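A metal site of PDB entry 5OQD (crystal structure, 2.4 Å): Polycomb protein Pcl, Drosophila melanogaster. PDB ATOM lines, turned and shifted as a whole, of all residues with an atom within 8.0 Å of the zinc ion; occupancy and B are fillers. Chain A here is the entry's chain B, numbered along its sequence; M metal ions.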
ATOM      1  N   GLN A  44     -24.517   2.926 -15.764  1.00  0.00           N
ATOM      2  CA  GLN A  44     -24.929   1.571 -16.138  1.00  0.00           C
ATOM      3  C   GLN A  44     -23.820   0.874 -16.925  1.00  0.00           C
ATOM      4  O   GLN A  44     -23.267   1.450 -17.868  1.00  0.00           O
ATOM      5  CB  GLN A  44     -26.221   1.597 -16.953  1.00  0.00           C
ATOM      6  CG  GLN A  44     -26.779   0.227 -17.269  1.00  0.00           C
ATOM      7  CD  GLN A  44     -28.042   0.297 -18.113  1.00  0.00           C
ATOM      8  OE1 GLN A  44     -28.261   1.256 -18.846  1.00  0.00           O
ATOM      9  NE2 GLN A  44     -28.884  -0.725 -17.987  1.00  0.00           N
ATOM     10  N   CYS A  45     -23.491  -0.355 -16.538  1.00  0.00           N
ATOM     11  CA  CYS A  45     -22.473  -1.125 -17.240  1.00  0.00           C
ATOM     12  C   CYS A  45     -22.965  -1.478 -18.642  1.00  0.00           C
ATOM     13  O   CYS A  45     -24.115  -1.878 -18.834  1.00  0.00           O
ATOM     14  CB  CYS A  45     -22.132  -2.393 -16.463  1.00  0.00           C
ATOM     15  SG  CYS A  45     -20.891  -3.455 -17.255  1.00  0.00           S
ATOM     16  N   CYS A  46     -22.107  -1.313 -19.630  1.00  0.00           N
ATOM     17  CA  CYS A  46     -22.474  -1.702 -20.980  1.00  0.00           C
ATOM     18  C   CYS A  46     -22.698  -3.195 -21.201  1.00  0.00           C
ATOM     19  O   CYS A  46     -23.561  -3.564 -21.963  1.00  0.00           O
ATOM     20  CB  CYS A  46     -21.535  -1.090 -22.027  1.00  0.00           C
ATOM     21  SG  CYS A  46     -19.794  -1.457 -21.863  1.00  0.00           S
ATOM     22  N   LYS A  47     -21.863  -4.050 -20.625  1.00  0.00           N
ATOM     23  CA  LYS A  47     -22.108  -5.493 -20.689  1.00  0.00           C
ATOM     24  C   LYS A  47     -23.219  -6.186 -19.866  1.00  0.00           C
ATOM     25  O   LYS A  47     -24.004  -6.932 -20.415  1.00  0.00           O
ATOM     26  CB  LYS A  47     -20.770  -6.231 -20.567  1.00  0.00           C
ATOM     27  CG  LYS A  47     -19.833  -5.890 -21.704  1.00  0.00           C
ATOM     28  CD  LYS A  47     -18.481  -6.560 -21.560  1.00  0.00           C
ATOM     29  CE  LYS A  47     -17.955  -7.011 -22.900  1.00  0.00           C
ATOM     30  NZ  LYS A  47     -16.487  -7.187 -22.881  1.00  0.00           N
ATOM     31  N   CYS A  48     -23.314  -5.895 -18.575  1.00  0.00           N
ATOM     32  CA  CYS A  48     -24.264  -6.556 -17.685  1.00  0.00           C
ATOM     33  C   CYS A  48     -25.520  -5.719 -17.489  1.00  0.00           C
ATOM     34  O   CYS A  48     -26.552  -6.223 -17.026  1.00  0.00           O
ATOM     35  CB  CYS A  48     -23.609  -6.854 -16.336  1.00  0.00           C
ATOM     36  SG  CYS A  48     -23.156  -5.402 -15.356  1.00  0.00           S
ATOM     37  N   ARG A  49     -25.428  -4.443 -17.849  1.00  0.00           N
ATOM     38  CA  ARG A  49     -26.557  -3.505 -17.832  1.00  0.00           C
ATOM     39  C   ARG A  49     -27.107  -3.259 -16.419  1.00  0.00           C
ATOM     40  O   ARG A  49     -28.259  -2.834 -16.265  1.00  0.00           O
ATOM     41  CB  ARG A  49     -27.673  -3.998 -18.761  1.00  0.00           C
ATOM     42  CG  ARG A  49     -27.168  -4.390 -20.141  1.00  0.00           C
ATOM     43  CD  ARG A  49     -28.276  -4.872 -21.044  1.00  0.00           C
ATOM     44  NE  ARG A  49     -27.729  -5.445 -22.282  1.00  0.00           N
ATOM     45  CZ  ARG A  49     -28.462  -5.995 -23.241  1.00  0.00           C
ATOM     46  NH1 ARG A  49     -29.784  -6.041 -23.113  1.00  0.00           N
ATOM     47  NH2 ARG A  49     -27.881  -6.500 -24.314  1.00  0.00           N
ATOM     48  N   ASN A  50     -26.286  -3.515 -15.409  1.00  0.00           N
ATOM     49  CA  ASN A  50     -26.627  -3.175 -14.041  1.00  0.00           C
ATOM     50  C   ASN A  50     -26.166  -1.752 -13.725  1.00  0.00           C
ATOM     51  O   ASN A  50     -25.281  -1.221 -14.376  1.00  0.00           O
ATOM     52  CB  ASN A  50     -26.005  -4.162 -13.060  1.00  0.00           C
ATOM     53  CG  ASN A  50     -26.681  -5.510 -13.081  1.00  0.00           C
ATOM     54  OD1 ASN A  50     -27.915  -5.611 -13.177  1.00  0.00           O
ATOM     55  ND2 ASN A  50     -25.898  -6.580 -13.002  1.00  0.00           N
ATOM     56  N   TRP A  51     -26.781  -1.142 -12.708  1.00  0.00           N
ATOM     57  CA  TRP A  51     -26.424   0.210 -12.314  1.00  0.00           C
ATOM     58  C   TRP A  51     -25.468   0.198 -11.124  1.00  0.00           C
ATOM     59  O   TRP A  51     -25.560  -0.658 -10.246  1.00  0.00           O
ATOM     60  CB  TRP A  51     -27.669   1.036 -12.002  1.00  0.00           C
ATOM     61  CG  TRP A  51     -28.561   1.222 -13.186  1.00  0.00           C
ATOM     62  CD1 TRP A  51     -29.521   0.370 -13.640  1.00  0.00           C
ATOM     63  CD2 TRP A  51     -28.577   2.340 -14.092  1.00  0.00           C
ATOM     64  NE1 TRP A  51     -30.128   0.881 -14.754  1.00  0.00           N
ATOM     65  CE2 TRP A  51     -29.565   2.091 -15.056  1.00  0.00           C
ATOM     66  CE3 TRP A  51     -27.838   3.529 -14.174  1.00  0.00           C
ATOM     67  CZ2 TRP A  51     -29.846   2.983 -16.081  1.00  0.00           C
ATOM     68  CZ3 TRP A  51     -28.113   4.408 -15.195  1.00  0.00           C
ATOM     69  CH2 TRP A  51     -29.109   4.139 -16.137  1.00  0.00           C
ATOM     70  N   PHE A  52     -24.546   1.160 -11.104  1.00  0.00           N
ATOM     71  CA  PHE A  52     -23.524   1.210 -10.078  1.00  0.00           C
ATOM     72  C   PHE A  52     -23.397   2.607  -9.474  1.00  0.00           C
ATOM     73  O   PHE A  52     -23.448   3.604 -10.191  1.00  0.00           O
ATOM     74  CB  PHE A  52     -22.155   0.794 -10.654  1.00  0.00           C
ATOM     75  CG  PHE A  52     -22.099  -0.640 -11.101  1.00  0.00           C
ATOM     76  CD1 PHE A  52     -22.656  -1.040 -12.311  1.00  0.00           C
ATOM     77  CD2 PHE A  52     -21.464  -1.589 -10.323  1.00  0.00           C
ATOM     78  CE1 PHE A  52     -22.580  -2.353 -12.725  1.00  0.00           C
ATOM     79  CE2 PHE A  52     -21.391  -2.911 -10.732  1.00  0.00           C
ATOM     80  CZ  PHE A  52     -21.951  -3.294 -11.938  1.00  0.00           C
ATOM     81  N   PHE A  73     -19.193   2.851 -19.607  1.00  0.00           N
ATOM     82  CA  PHE A  73     -18.694   2.151 -18.432  1.00  0.00           C
ATOM     83  C   PHE A  73     -18.863   0.639 -18.515  1.00  0.00           C
ATOM     84  O   PHE A  73     -19.902   0.138 -18.931  1.00  0.00           O
ATOM     85  CB  PHE A  73     -19.397   2.676 -17.176  1.00  0.00           C
ATOM     86  CG  PHE A  73     -19.133   1.874 -15.944  1.00  0.00           C
ATOM     87  CD1 PHE A  73     -17.842   1.714 -15.471  1.00  0.00           C
ATOM     88  CD2 PHE A  73     -20.175   1.267 -15.262  1.00  0.00           C
ATOM     89  CE1 PHE A  73     -17.598   0.964 -14.333  1.00  0.00           C
ATOM     90  CE2 PHE A  73     -19.932   0.517 -14.125  1.00  0.00           C
ATOM     91  CZ  PHE A  73     -18.641   0.362 -13.665  1.00  0.00           C
ATOM     92  N   CYS A  74     -17.815  -0.077 -18.119  1.00  0.00           N
ATOM     93  CA  CYS A  74     -17.869  -1.529 -17.994  1.00  0.00           C
ATOM     94  C   CYS A  74     -17.269  -1.935 -16.660  1.00  0.00           C
ATOM     95  O   CYS A  74     -16.119  -1.607 -16.358  1.00  0.00           O
ATOM     96  CB  CYS A  74     -17.138  -2.205 -19.150  1.00  0.00           C
ATOM     97  SG  CYS A  74     -17.420  -3.981 -19.263  1.00  0.00           S
ATOM     98  N   CYS A  75     -18.061  -2.637 -15.854  1.00  0.00           N
ATOM     99  CA  CYS A  75     -17.649  -2.974 -14.495  1.00  0.00           C
ATOM    100  C   CYS A  75     -16.538  -4.027 -14.468  1.00  0.00           C
ATOM    101  O   CYS A  75     -16.221  -4.620 -15.503  1.00  0.00           O
ATOM    102  CB  CYS A  75     -18.846  -3.476 -13.679  1.00  0.00           C
ATOM    103  SG  CYS A  75     -19.464  -5.101 -14.162  1.00  0.00           S
ATOM    104  N   THR A  76     -15.980  -4.248 -13.290  1.00  0.00           N
ATOM    105  CA  THR A  76     -14.862  -5.170 -13.116  1.00  0.00           C
ATOM    106  C   THR A  76     -15.272  -6.631 -13.331  1.00  0.00           C
ATOM    107  O   THR A  76     -14.429  -7.485 -13.604  1.00  0.00           O
ATOM    108  CB  THR A  76     -14.244  -5.035 -11.723  1.00  0.00           C
ATOM    109  OG1 THR A  76     -15.259  -5.201 -10.725  1.00  0.00           O
ATOM    110  CG2 THR A  76     -13.614  -3.659 -11.560  1.00  0.00           C
ATOM    111  N   VAL A  77     -16.565  -6.915 -13.191  1.00  0.00           N
ATOM    112  CA  VAL A  77     -17.067  -8.275 -13.382  1.00  0.00           C
ATOM    113  C   VAL A  77     -17.089  -8.654 -14.870  1.00  0.00           C
ATOM    114  O   VAL A  77     -16.746  -9.783 -15.238  1.00  0.00           O
ATOM    115  CB  VAL A  77     -18.488  -8.438 -12.804  1.00  0.00           C
ATOM    116  CG1 VAL A  77     -18.990  -9.867 -12.988  1.00  0.00           C
ATOM    117  CG2 VAL A  77     -18.508  -8.049 -11.329  1.00  0.00           C
ATOM    118  N   CYS A  78     -17.484  -7.705 -15.708  1.00  0.00           N
ATOM    119  CA  CYS A  78     -17.637  -7.957 -17.135  1.00  0.00           C
ATOM    120  C   CYS A  78     -16.352  -7.713 -17.929  1.00  0.00           C
ATOM    121  O   CYS A  78     -16.263  -8.092 -19.100  1.00  0.00           O
ATOM    122  CB  CYS A  78     -18.760  -7.074 -17.701  1.00  0.00           C
ATOM    123  SG  CYS A  78     -20.383  -7.311 -16.929  1.00  0.00           S
ATOM    124  N   ASN A  79     -15.368  -7.088 -17.295  1.00  0.00           N
ATOM    125  CA  ASN A  79     -14.138  -6.709 -18.002  1.00  0.00           C
ATOM    126  C   ASN A  79     -12.876  -7.289 -17.362  1.00  0.00           C
ATOM    127  O   ASN A  79     -11.853  -6.615 -17.277  1.00  0.00           O
ATOM    128  CB  ASN A  79     -14.033  -5.187 -18.095  1.00  0.00           C
ATOM    129  CG  ASN A  79     -13.085  -4.725 -19.184  1.00  0.00           C
ATOM    130  OD1 ASN A  79     -12.986  -5.341 -20.247  1.00  0.00           O
ATOM    131  ND2 ASN A  79     -12.364  -3.647 -18.915  1.00  0.00           N
HETATM  132 ZN    ZN M   1     -20.938  -5.352 -15.869  1.00  0.00          ZN
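The zinc ion is bound by SG of Cys 75, 2.3 Å away. The zinc ion is bound by the side-chain sulfur (SG) of Cys 48 (2.3 Å). SG of Cys 78 is bound to the zinc ion (2.3 Å). SG of Cys 45 is bound to the zinc ion (2.3 Å). The zinc ion has four donor atoms within binding distance.
Along chain A the residues within 4 Å of the zinc ion span positions 45 to 78. The nearest printed residue that does not touch the zinc ion is Phe 52 (4.6 Å).
SG of Cys 75 sits close to N of Val 77, 3.6 Å away. The side-chain sulfur (SG) of Cys 48 sits close to the backbone NH (N) of Asn 50. The side-chain sulfur of Cys 45 sits close to the backbone NH of Lys 47 (3.6 Å). The backbone NH (N) of Cys 45 sits at hydrogen-bond distance from the backbone carbonyl oxygen (O) of Asn 50 (2.9 Å).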
